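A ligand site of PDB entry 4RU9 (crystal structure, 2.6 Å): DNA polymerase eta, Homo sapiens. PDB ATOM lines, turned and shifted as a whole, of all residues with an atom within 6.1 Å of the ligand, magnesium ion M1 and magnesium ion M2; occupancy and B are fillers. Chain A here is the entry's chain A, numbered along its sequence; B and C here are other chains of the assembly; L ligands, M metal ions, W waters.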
ATOM      1  N   ASP A  13     -15.846 -30.068  11.394  1.00  0.00           N
ATOM      2  CA  ASP A  13     -16.782 -30.015  12.475  1.00  0.00           C
ATOM      3  C   ASP A  13     -17.711 -31.216  12.358  1.00  0.00           C
ATOM      4  O   ASP A  13     -18.235 -31.520  11.294  1.00  0.00           O
ATOM      5  CB  ASP A  13     -17.606 -28.716  12.434  1.00  0.00           C
ATOM      6  CG  ASP A  13     -18.588 -28.603  13.620  1.00  0.00           C
ATOM      7  OD1 ASP A  13     -18.334 -27.803  14.554  1.00  0.00           O
ATOM      8  OD2 ASP A  13     -19.595 -29.354  13.660  1.00  0.00           O
ATOM      9  N   MET A  14     -17.955 -31.862  13.474  1.00  0.00           N
ATOM     10  CA  MET A  14     -18.784 -33.034  13.489  1.00  0.00           C
ATOM     11  C   MET A  14     -20.259 -32.626  13.379  1.00  0.00           C
ATOM     12  O   MET A  14     -20.689 -31.594  13.926  1.00  0.00           O
ATOM     13  CB  MET A  14     -18.558 -33.859  14.761  1.00  0.00           C
ATOM     14  CG  MET A  14     -17.096 -34.132  15.082  1.00  0.00           C
ATOM     15  SD  MET A  14     -16.184 -34.936  13.782  1.00  0.00           S
ATOM     16  CE  MET A  14     -16.969 -36.525  13.892  1.00  0.00           C
ATOM     17  N   ASP A  15     -21.001 -33.457  12.677  1.00  0.00           N
ATOM     18  CA  ASP A  15     -22.441 -33.280  12.565  1.00  0.00           C
ATOM     19  C   ASP A  15     -23.110 -33.669  13.871  1.00  0.00           C
ATOM     20  O   ASP A  15     -22.830 -34.721  14.442  1.00  0.00           O
ATOM     21  CB  ASP A  15     -22.959 -34.063  11.355  1.00  0.00           C
ATOM     22  CG  ASP A  15     -22.242 -33.674  10.062  1.00  0.00           C
ATOM     23  OD1 ASP A  15     -21.738 -32.525   9.981  1.00  0.00           O
ATOM     24  OD2 ASP A  15     -22.171 -34.495   9.119  1.00  0.00           O
ATOM     25  N   CYS A  16     -24.021 -32.813  14.334  1.00  0.00           N
ATOM     26  CA  CYS A  16     -24.763 -33.019  15.589  1.00  0.00           C
ATOM     27  C   CYS A  16     -23.983 -33.902  16.580  1.00  0.00           C
ATOM     28  O   CYS A  16     -24.379 -35.010  16.857  1.00  0.00           O
ATOM     29  CB  CYS A  16     -26.148 -33.591  15.279  1.00  0.00           C
ATOM     30  SG  CYS A  16     -26.125 -35.023  14.201  1.00  0.00           S
ATOM     31  N   PHE A  17     -22.855 -33.422  17.076  1.00  0.00           N
ATOM     32  CA  PHE A  17     -21.884 -34.348  17.608  1.00  0.00           C
ATOM     33  C   PHE A  17     -22.356 -35.262  18.765  1.00  0.00           C
ATOM     34  O   PHE A  17     -22.284 -36.517  18.693  1.00  0.00           O
ATOM     35  CB  PHE A  17     -20.674 -33.570  18.038  1.00  0.00           C
ATOM     36  CG  PHE A  17     -19.561 -34.423  18.487  1.00  0.00           C
ATOM     37  CD1 PHE A  17     -19.135 -35.461  17.700  1.00  0.00           C
ATOM     38  CD2 PHE A  17     -18.978 -34.229  19.726  1.00  0.00           C
ATOM     39  CE1 PHE A  17     -18.121 -36.303  18.134  1.00  0.00           C
ATOM     40  CE2 PHE A  17     -17.951 -35.054  20.164  1.00  0.00           C
ATOM     41  CZ  PHE A  17     -17.520 -36.091  19.358  1.00  0.00           C
ATOM     42  N   PHE A  18     -22.870 -34.644  19.830  1.00  0.00           N
ATOM     43  CA  PHE A  18     -23.335 -35.385  20.986  1.00  0.00           C
ATOM     44  C   PHE A  18     -24.395 -36.410  20.585  1.00  0.00           C
ATOM     45  O   PHE A  18     -24.427 -37.503  21.145  1.00  0.00           O
ATOM     46  CB  PHE A  18     -23.874 -34.423  22.029  1.00  0.00           C
ATOM     47  CG  PHE A  18     -22.803 -33.629  22.774  1.00  0.00           C
ATOM     48  CD1 PHE A  18     -21.526 -33.459  22.291  1.00  0.00           C
ATOM     49  CD2 PHE A  18     -23.125 -32.990  23.973  1.00  0.00           C
ATOM     50  CE1 PHE A  18     -20.578 -32.699  22.992  1.00  0.00           C
ATOM     51  CE2 PHE A  18     -22.184 -32.249  24.681  1.00  0.00           C
ATOM     52  CZ  PHE A  18     -20.908 -32.099  24.186  1.00  0.00           C
ATOM     53  N   VAL A  19     -25.234 -36.079  19.603  1.00  0.00           N
ATOM     54  CA  VAL A  19     -26.271 -36.997  19.119  1.00  0.00           C
ATOM     55  C   VAL A  19     -25.613 -38.239  18.488  1.00  0.00           C
ATOM     56  O   VAL A  19     -25.956 -39.382  18.818  1.00  0.00           O
ATOM     57  CB  VAL A  19     -27.251 -36.291  18.139  1.00  0.00           C
ATOM     58  CG1 VAL A  19     -28.092 -37.280  17.363  1.00  0.00           C
ATOM     59  CG2 VAL A  19     -28.174 -35.307  18.886  1.00  0.00           C
ATOM     60  N   ILE A  48     -29.271 -29.777  24.278  1.00  0.00           N
ATOM     61  CA  ILE A  48     -27.926 -29.333  23.888  1.00  0.00           C
ATOM     62  C   ILE A  48     -27.452 -29.811  22.520  1.00  0.00           C
ATOM     63  O   ILE A  48     -26.527 -29.249  21.973  1.00  0.00           O
ATOM     64  CB  ILE A  48     -26.889 -29.651  24.974  1.00  0.00           C
ATOM     65  CG1 ILE A  48     -26.573 -31.124  25.080  1.00  0.00           C
ATOM     66  CG2 ILE A  48     -27.407 -29.185  26.340  1.00  0.00           C
ATOM     67  CD1 ILE A  48     -25.453 -31.358  26.078  1.00  0.00           C
ATOM     68  N   ALA A  49     -28.101 -30.804  21.938  1.00  0.00           N
ATOM     69  CA  ALA A  49     -27.776 -31.182  20.577  1.00  0.00           C
ATOM     70  C   ALA A  49     -28.960 -31.874  19.952  1.00  0.00           C
ATOM     71  O   ALA A  49     -29.663 -32.605  20.642  1.00  0.00           O
ATOM     72  CB  ALA A  49     -26.543 -32.064  20.570  1.00  0.00           C
ATOM     73  N   VAL A  50     -29.179 -31.631  18.653  1.00  0.00           N
ATOM     74  CA  VAL A  50     -30.380 -32.053  17.912  1.00  0.00           C
ATOM     75  C   VAL A  50     -29.961 -32.774  16.632  1.00  0.00           C
ATOM     76  O   VAL A  50     -29.095 -32.278  15.931  1.00  0.00           O
ATOM     77  CB  VAL A  50     -31.235 -30.844  17.497  1.00  0.00           C
ATOM     78  CG1 VAL A  50     -32.636 -31.256  17.056  1.00  0.00           C
ATOM     79  CG2 VAL A  50     -31.311 -29.855  18.611  1.00  0.00           C
ATOM     80  N   TYR A  52     -30.435 -34.002  12.700  1.00  0.00           N
ATOM     81  CA  TYR A  52     -31.005 -33.335  11.526  1.00  0.00           C
ATOM     82  C   TYR A  52     -32.462 -33.744  11.267  1.00  0.00           C
ATOM     83  O   TYR A  52     -33.285 -32.924  10.893  1.00  0.00           O
ATOM     84  CB  TYR A  52     -30.088 -33.481  10.280  1.00  0.00           C
ATOM     85  CG  TYR A  52     -28.871 -32.560  10.387  1.00  0.00           C
ATOM     86  CD1 TYR A  52     -27.780 -32.902  11.196  1.00  0.00           C
ATOM     87  CD2 TYR A  52     -28.854 -31.315   9.768  1.00  0.00           C
ATOM     88  CE1 TYR A  52     -26.666 -32.073  11.302  1.00  0.00           C
ATOM     89  CE2 TYR A  52     -27.751 -30.465   9.892  1.00  0.00           C
ATOM     90  CZ  TYR A  52     -26.658 -30.835  10.670  1.00  0.00           C
ATOM     91  OH  TYR A  52     -25.578 -29.964  10.821  1.00  0.00           O
ATOM     92  N   ARG A  55     -34.287 -31.416  13.527  1.00  0.00           N
ATOM     93  CA  ARG A  55     -34.206 -30.016  13.078  1.00  0.00           C
ATOM     94  C   ARG A  55     -35.293 -29.715  12.050  1.00  0.00           C
ATOM     95  O   ARG A  55     -35.850 -28.623  12.029  1.00  0.00           O
ATOM     96  CB  ARG A  55     -32.841 -29.710  12.490  1.00  0.00           C
ATOM     97  CG  ARG A  55     -31.753 -29.687  13.544  1.00  0.00           C
ATOM     98  CD  ARG A  55     -30.371 -29.487  12.965  1.00  0.00           C
ATOM     99  NE  ARG A  55     -29.319 -29.981  13.840  1.00  0.00           N
ATOM    100  CZ  ARG A  55     -28.042 -29.593  13.833  1.00  0.00           C
ATOM    101  NH1 ARG A  55     -27.560 -28.730  12.967  1.00  0.00           N
ATOM    102  NH2 ARG A  55     -27.226 -30.145  14.716  1.00  0.00           N
ATOM    103  N   ARG A  61     -31.320 -26.321  19.939  1.00  0.00           N
ATOM    104  CA  ARG A  61     -30.624 -26.078  21.190  1.00  0.00           C
ATOM    105  C   ARG A  61     -31.373 -24.984  21.926  1.00  0.00           C
ATOM    106  O   ARG A  61     -32.056 -24.183  21.277  1.00  0.00           O
ATOM    107  CB  ARG A  61     -29.198 -25.639  20.894  1.00  0.00           C
ATOM    108  CG  ARG A  61     -28.276 -25.628  22.090  1.00  0.00           C
ATOM    109  CD  ARG A  61     -26.803 -25.710  21.698  1.00  0.00           C
ATOM    110  NE  ARG A  61     -26.512 -25.064  20.398  1.00  0.00           N
ATOM    111  CZ  ARG A  61     -26.072 -25.694  19.283  1.00  0.00           C
ATOM    112  NH1 ARG A  61     -25.828 -27.004  19.232  1.00  0.00           N
ATOM    113  NH2 ARG A  61     -25.858 -24.962  18.194  1.00  0.00           N
ATOM    114  N   SER A 113     -12.752 -26.725  19.338  1.00  0.00           N
ATOM    115  CA  SER A 113     -13.886 -26.964  20.239  1.00  0.00           C
ATOM    116  C   SER A 113     -13.817 -28.443  20.569  1.00  0.00           C
ATOM    117  O   SER A 113     -12.888 -29.141  20.128  1.00  0.00           O
ATOM    118  CB  SER A 113     -15.230 -26.617  19.560  1.00  0.00           C
ATOM    119  OG  SER A 113     -15.805 -27.719  18.796  1.00  0.00           O
ATOM    120  N   ILE A 114     -14.797 -28.940  21.301  1.00  0.00           N
ATOM    121  CA  ILE A 114     -14.865 -30.369  21.504  1.00  0.00           C
ATOM    122  C   ILE A 114     -15.136 -31.153  20.235  1.00  0.00           C
ATOM    123  O   ILE A 114     -14.723 -32.299  20.155  1.00  0.00           O
ATOM    124  CB  ILE A 114     -15.898 -30.754  22.549  1.00  0.00           C
ATOM    125  CG1 ILE A 114     -15.680 -32.200  22.982  1.00  0.00           C
ATOM    126  CG2 ILE A 114     -17.305 -30.526  22.054  1.00  0.00           C
ATOM    127  CD1 ILE A 114     -16.557 -32.565  24.131  1.00  0.00           C
ATOM    128  N   ASP A 115     -15.778 -30.530  19.227  1.00  0.00           N
ATOM    129  CA  ASP A 115     -16.131 -31.238  17.971  1.00  0.00           C
ATOM    130  C   ASP A 115     -15.526 -30.675  16.688  1.00  0.00           C
ATOM    131  O   ASP A 115     -15.897 -31.120  15.605  1.00  0.00           O
ATOM    132  CB  ASP A 115     -17.665 -31.378  17.829  1.00  0.00           C
ATOM    133  CG  ASP A 115     -18.307 -30.279  16.978  1.00  0.00           C
ATOM    134  OD1 ASP A 115     -17.977 -29.073  17.174  1.00  0.00           O
ATOM    135  OD2 ASP A 115     -19.202 -30.598  16.157  1.00  0.00           O
ATOM    136  N   GLU A 116     -14.602 -29.716  16.781  1.00  0.00           N
ATOM    137  CA  GLU A 116     -13.960 -29.211  15.597  1.00  0.00           C
ATOM    138  C   GLU A 116     -12.494 -28.857  15.773  1.00  0.00           C
ATOM    139  O   GLU A 116     -12.048 -28.540  16.869  1.00  0.00           O
ATOM    140  CB  GLU A 116     -14.732 -28.035  15.036  1.00  0.00           C
ATOM    141  CG  GLU A 116     -14.725 -26.802  15.905  1.00  0.00           C
ATOM    142  CD  GLU A 116     -16.003 -26.009  15.762  1.00  0.00           C
ATOM    143  OE1 GLU A 116     -15.961 -25.005  15.045  1.00  0.00           O
ATOM    144  OE2 GLU A 116     -17.048 -26.398  16.348  1.00  0.00           O
ATOM    145  N   LYS A 231     -23.557 -28.464   5.380  1.00  0.00           N
ATOM    146  CA  LYS A 231     -23.832 -29.473   6.387  1.00  0.00           C
ATOM    147  C   LYS A 231     -25.158 -30.145   6.047  1.00  0.00           C
ATOM    148  O   LYS A 231     -26.042 -29.449   5.599  1.00  0.00           O
ATOM    149  CB  LYS A 231     -23.932 -28.822   7.759  1.00  0.00           C
ATOM    150  CG  LYS A 231     -22.598 -28.622   8.410  1.00  0.00           C
ATOM    151  CD  LYS A 231     -22.704 -28.350   9.896  1.00  0.00           C
ATOM    152  CE  LYS A 231     -21.391 -28.603  10.613  1.00  0.00           C
ATOM    153  NZ  LYS A 231     -21.254 -30.048  10.994  1.00  0.00           N
ATOM    154  N   PRO A 232     -25.341 -31.442   6.277  1.00  0.00           N
ATOM    155  CA  PRO A 232     -24.409 -32.352   6.935  1.00  0.00           C
ATOM    156  C   PRO A 232     -23.670 -33.292   5.997  1.00  0.00           C
ATOM    157  O   PRO A 232     -24.118 -33.568   4.903  1.00  0.00           O
ATOM    158  CB  PRO A 232     -25.340 -33.190   7.808  1.00  0.00           C
ATOM    159  CG  PRO A 232     -26.627 -33.246   7.052  1.00  0.00           C
ATOM    160  CD  PRO A 232     -26.745 -31.883   6.445  1.00  0.00           C
ATOM    161  P    DT B   8     -19.655 -21.058  17.212  1.00  0.00           P
ATOM    162  OP1  DT B   8     -19.577 -21.517  15.803  1.00  0.00           O
ATOM    163  OP2  DT B   8     -20.927 -20.476  17.743  1.00  0.00           O
ATOM    164  O5'  DT B   8     -19.285 -22.296  18.140  1.00  0.00           O
ATOM    165  C5'  DT B   8     -18.054 -23.020  17.985  1.00  0.00           C
ATOM    166  C4'  DT B   8     -18.081 -24.220  18.893  1.00  0.00           C
ATOM    167  O4'  DT B   8     -18.249 -23.781  20.267  1.00  0.00           O
ATOM    168  C3'  DT B   8     -19.231 -25.187  18.605  1.00  0.00           C
ATOM    169  O3'  DT B   8     -18.837 -26.563  18.611  1.00  0.00           O
ATOM    170  C2'  DT B   8     -20.215 -24.955  19.734  1.00  0.00           C
ATOM    171  C1'  DT B   8     -19.349 -24.457  20.866  1.00  0.00           C
ATOM    172  N1   DT B   8     -20.034 -23.504  21.767  1.00  0.00           N
ATOM    173  C2   DT B   8     -20.167 -23.806  23.115  1.00  0.00           C
ATOM    174  O2   DT B   8     -19.747 -24.837  23.611  1.00  0.00           O
ATOM    175  N3   DT B   8     -20.830 -22.860  23.845  1.00  0.00           N
ATOM    176  C4   DT B   8     -21.349 -21.651  23.394  1.00  0.00           C
ATOM    177  O4   DT B   8     -21.920 -20.892  24.181  1.00  0.00           O
ATOM    178  C5   DT B   8     -21.169 -21.402  21.983  1.00  0.00           C
ATOM    179  C7   DT B   8     -21.725 -20.132  21.401  1.00  0.00           C
ATOM    180  C6   DT B   8     -20.544 -22.331  21.254  1.00  0.00           C
ATOM    181  P    DT C   3     -33.387 -19.262  30.481  1.00  0.00           P
ATOM    182  OP1  DT C   3     -33.827 -17.857  30.682  1.00  0.00           O
ATOM    183  OP2  DT C   3     -33.463 -19.903  29.147  1.00  0.00           O
ATOM    184  O5'  DT C   3     -31.890 -19.369  31.016  1.00  0.00           O
ATOM    185  C5'  DT C   3     -31.022 -20.422  30.552  1.00  0.00           C
ATOM    186  C4'  DT C   3     -31.728 -21.755  30.612  1.00  0.00           C
ATOM    187  O4'  DT C   3     -31.842 -22.350  29.300  1.00  0.00           O
ATOM    188  C3'  DT C   3     -31.028 -22.820  31.428  1.00  0.00           C
ATOM    189  O3'  DT C   3     -31.227 -22.666  32.843  1.00  0.00           O
ATOM    190  C2'  DT C   3     -31.747 -24.056  30.952  1.00  0.00           C
ATOM    191  C1'  DT C   3     -31.983 -23.771  29.464  1.00  0.00           C
ATOM    192  N1   DT C   3     -31.026 -24.449  28.555  1.00  0.00           N
ATOM    193  C2   DT C   3     -30.632 -25.741  28.845  1.00  0.00           C
ATOM    194  O2   DT C   3     -31.036 -26.354  29.827  1.00  0.00           O
ATOM    195  N3   DT C   3     -29.748 -26.285  27.965  1.00  0.00           N
ATOM    196  C4   DT C   3     -29.225 -25.690  26.827  1.00  0.00           C
ATOM    197  O4   DT C   3     -28.435 -26.315  26.125  1.00  0.00           O
ATOM    198  C5   DT C   3     -29.680 -24.349  26.575  1.00  0.00           C
ATOM    199  C7   DT C   3     -29.136 -23.620  25.387  1.00  0.00           C
ATOM    200  C6   DT C   3     -30.547 -23.806  27.429  1.00  0.00           C
ATOM    201  P1  MF7 C   4     -29.719 -22.680  33.665  1.00  0.00           P
ATOM    202  OP1 MF7 C   4     -29.821 -23.079  35.099  1.00  0.00           O
ATOM    203  O5' MF7 C   4     -29.009 -23.871  32.832  1.00  0.00           O
ATOM    204  C5' MF7 C   4     -29.205 -25.287  33.053  1.00  0.00           C
ATOM    205  C4' MF7 C   4     -27.901 -26.005  32.700  1.00  0.00           C
ATOM    206  C3' MF7 C   4     -26.773 -25.477  33.530  1.00  0.00           C
ATOM    207  O3' MF7 C   4     -26.082 -26.598  33.999  1.00  0.00           O
ATOM    208  C2' MF7 C   4     -25.975 -24.625  32.570  1.00  0.00           C
ATOM    209  C1' MF7 C   4     -26.275 -25.210  31.210  1.00  0.00           C
ATOM    210  O4' MF7 C   4     -27.568 -25.790  31.317  1.00  0.00           O
ATOM    211  N9  MF7 C   4     -26.219 -24.195  30.156  1.00  0.00           N
ATOM    212  C4  MF7 C   4     -25.720 -24.465  28.908  1.00  0.00           C
ATOM    213  C5  MF7 C   4     -25.731 -23.464  27.814  1.00  0.00           C
ATOM    214  N7  MF7 C   4     -26.197 -22.140  27.962  1.00  0.00           N
ATOM    215  C8  MF7 C   4     -27.425 -21.878  28.127  1.00  0.00           C
ATOM    216  N3  MF7 C   4     -25.208 -25.691  28.621  1.00  0.00           N
ATOM    217  C2  MF7 C   4     -24.723 -26.033  27.407  1.00  0.00           C
ATOM    218  N2  MF7 C   4     -24.257 -27.279  27.201  1.00  0.00           N
ATOM    219  N1  MF7 C   4     -24.722 -25.175  26.393  1.00  0.00           N
ATOM    220  C6  MF7 C   4     -25.174 -23.923  26.510  1.00  0.00           C
ATOM    221  O6  MF7 C   4     -25.138 -23.176  25.510  1.00  0.00           O
ATOM    222  OP2 MF7 C   4     -29.164 -21.335  33.255  1.00  0.00           O
ATOM    223  C3  MF7 C   4     -25.217 -21.054  27.900  1.00  0.00           C
ATOM    224  O4  MF7 C   4     -27.829 -20.717  28.139  1.00  0.00           O
ATOM    225  P    DA C   5     -24.755 -26.175  34.784  1.00  0.00           P
ATOM    226  OP1  DA C   5     -25.192 -27.309  35.618  1.00  0.00           O
ATOM    227  OP2  DA C   5     -24.491 -24.875  35.403  1.00  0.00           O
ATOM    228  O5'  DA C   5     -23.607 -26.592  33.762  1.00  0.00           O
ATOM    229  C5'  DA C   5     -23.693 -27.856  33.057  1.00  0.00           C
ATOM    230  C4'  DA C   5     -22.465 -28.142  32.208  1.00  0.00           C
ATOM    231  O4'  DA C   5     -22.505 -27.407  30.959  1.00  0.00           O
ATOM    232  C3'  DA C   5     -21.111 -27.812  32.850  1.00  0.00           C
ATOM    233  O3'  DA C   5     -20.272 -28.916  32.541  1.00  0.00           O
ATOM    234  C2'  DA C   5     -20.736 -26.491  32.215  1.00  0.00           C
ATOM    235  C1'  DA C   5     -21.318 -26.629  30.813  1.00  0.00           C
ATOM    236  N9   DA C   5     -21.669 -25.371  30.160  1.00  0.00           N
ATOM    237  C8   DA C   5     -22.263 -24.267  30.709  1.00  0.00           C
ATOM    238  N7   DA C   5     -22.426 -23.273  29.875  1.00  0.00           N
ATOM    239  C5   DA C   5     -21.905 -23.767  28.684  1.00  0.00           C
ATOM    240  C6   DA C   5     -21.772 -23.194  27.401  1.00  0.00           C
ATOM    241  N6   DA C   5     -22.184 -21.959  27.093  1.00  0.00           N
ATOM    242  N1   DA C   5     -21.214 -23.942  26.425  1.00  0.00           N
ATOM    243  C2   DA C   5     -20.802 -25.178  26.733  1.00  0.00           C
ATOM    244  N3   DA C   5     -20.847 -25.817  27.901  1.00  0.00           N
ATOM    245  C4   DA C   5     -21.422 -25.042  28.843  1.00  0.00           C
HETATM  246  P1  LIG L   1     -23.800 -29.295  13.827  1.00  0.00           P
HETATM  247  O1  LIG L   1     -24.702 -28.178  13.395  1.00  0.00           O
HETATM  248  O2  LIG L   1     -24.003 -30.416  12.829  1.00  0.00           O
HETATM  249  O3  LIG L   1     -22.356 -28.917  13.905  1.00  0.00           O
HETATM  250  P2  LIG L   1     -23.430 -29.895  16.474  1.00  0.00           P
HETATM  251  O4  LIG L   1     -22.104 -30.496  16.132  1.00  0.00           O
HETATM  252  O5  LIG L   1     -24.183 -30.669  17.490  1.00  0.00           O
HETATM  253  O6  LIG L   1     -24.317 -29.773  15.210  1.00  0.00           O
HETATM  254  P3  LIG L   1     -21.856 -27.592  17.321  1.00  0.00           P
HETATM  255  O7  LIG L   1     -20.920 -27.928  16.206  1.00  0.00           O
HETATM  256  O8  LIG L   1     -22.168 -26.112  17.455  1.00  0.00           O
HETATM  257  N1  LIG L   1     -23.270 -28.365  17.035  1.00  0.00           N
HETATM  258  O9  LIG L   1     -21.271 -28.116  18.682  1.00  0.00           O
HETATM  259  C1  LIG L   1     -20.910 -29.483  18.866  1.00  0.00           C
HETATM  260  C2  LIG L   1     -21.490 -30.055  20.083  1.00  0.00           C
HETATM  261  O10 LIG L   1     -21.026 -29.091  21.329  1.00  0.00           O
HETATM  262  C3  LIG L   1     -22.816 -30.080  20.136  1.00  0.00           C
HETATM  263  O11 LIG L   1     -23.273 -31.368  19.664  1.00  0.00           O
HETATM  264  C4  LIG L   1     -23.112 -30.061  21.654  1.00  0.00           C
HETATM  265  C5  LIG L   1     -21.992 -29.115  22.212  1.00  0.00           C
HETATM  266  N2  LIG L   1     -22.504 -27.813  22.357  1.00  0.00           N
HETATM  267  C6  LIG L   1     -22.998 -27.374  23.646  1.00  0.00           C
HETATM  268  N3  LIG L   1     -23.516 -26.037  23.760  1.00  0.00           N
HETATM  269  C7  LIG L   1     -23.571 -25.150  22.660  1.00  0.00           C
HETATM  270  C8  LIG L   1     -23.098 -25.594  21.366  1.00  0.00           C
HETATM  271  C9  LIG L   1     -22.578 -26.931  21.242  1.00  0.00           C
HETATM  272  O12 LIG L   1     -22.977 -28.079  24.621  1.00  0.00           O
HETATM  273  N4  LIG L   1     -24.096 -23.850  22.853  1.00  0.00           N
HETATM  274 MG    MG M   1     -20.727 -29.738  15.092  1.00  0.00          MG
HETATM  275 MG    MG M   2     -19.052 -27.328  16.427  1.00  0.00          MG
HETATM  276  O   HOH W   1     -19.623 -25.464  15.248  1.00  0.00           O
HETATM  277  O   HOH W   2     -26.864 -30.278  17.631  1.00  0.00           O
HETATM  278  O   HOH W   3     -25.332 -26.750  15.700  1.00  0.00           O
HETATM  279  O   HOH W   4     -22.773 -23.665  15.415  1.00  0.00           O
HETATM  280  O   HOH W   5     -21.796 -26.167  13.979  1.00  0.00           O
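An oxygen (O2) of the ligand lies within hydrogen-bond range of the backbone NH (N) of Cys 16 (2.8 Å). N of Phe 18 is in hydrogen-bond range of O11 of the ligand. O2 of the ligand is in salt-bridge range of NZ of Lys 231 (3.3 Å). The side-chain hydroxyl of Tyr 52 sits at hydrogen-bond distance from an oxygen (O2) of the ligand, 2.6 Å away. The guanidinium group (NH2) of Arg 61 is in salt-bridge range of an oxygen (O8) of the ligand (3.9 Å). The guanidinium group (NH1) of Arg 55 lies within salt-bridge range of an oxygen (O1) of the ligand (2.9 Å). The backbone NH (N) of Phe 17 is in hydrogen-bond range of an oxygen (O5) of the ligand, 3.1 Å away. O6 of MF7 4 of chain C is in hydrogen-bond range of a nitrogen (N4) of the ligand, at 2.9 Å.
Of the 23 residues printed, 3 come within 4 Å of magnesium ion M1. Along chain A the residues within 4 Å of magnesium ion M1 span positions 13 to 115. The nearest printed residue that does not touch magnesium ion M1 is Lys 231 (4.1 Å).
The nearest printed residue that does not touch magnesium ion M2 is Ser 113 (4.04 Å).
Magnesium ion M2 is bound by O7 of the ligand (2.0 Å), OD1 of Asp 13 (2.1 Å), OD1 of Asp 115 (2.2 Å), OE2 of Glu 116 (2.2 Å), water W1 (2.3 Å) and O3' of DT 8 of chain B (2.3 Å).
Water W2 lies within hydrogen-bond range of an oxygen (O5) of the ligand, the backbone NH (N) of Val 50 and the guanidinium group (NH2) of Arg 55. Water W3 lies within hydrogen-bond range of an oxygen (O1) of the ligand and the guanidinium group (NH2) of Arg 61.
NZ of Lys 231 is in hydrogen-bond range of O of Asp 13 (3.4 Å). The backbone NH (N) of Glu 116 lies within hydrogen-bond range of the side-chain hydroxyl (OG) of Ser 113. NH1 of Arg 55 lies within hydrogen-bond range of OH of Tyr 52 (3.2 Å). O of Val 50 is in hydrogen-bond range of NH2 of Arg 55, at 3.1 Å. OG of Ser 113 sits at hydrogen-bond distance from N of Asp 115 (2.8 Å). The side-chain amino group (NZ) of Lys 231 sits close to the backbone carbonyl oxygen (O) of Met 14 (3.4 Å). The side-chain hydroxyl (OG) of Ser 113 lies close to O3' of DT 8 of chain B (3.3 Å). The side-chain carboxylate (OD1) of Asp 15 lies within salt-bridge range of the side-chain amino group (NZ) of Lys 231 (2.7 Å).
Residues that only touch the ligand: Asp 15 (3.3 Å), Ile 48 (3.5 Å) and Ala 49 (3.5 Å). Hydrophobic or aromatic side chains that line the ligand: Phe 17, Phe 18, Ala 49 and Tyr 52.
Magnesium ion M1 is bound by OD2 of Asp 13 (1.9 Å), O4 of the ligand (1.9 Å), OD2 of Asp 115 (2.0 Å), O7 of the ligand (2.1 Å), O3 of the ligand (2.2 Å) and O of Met 14 (2.2 Å). Magnesium ion M1 has six donor atoms within binding distance.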
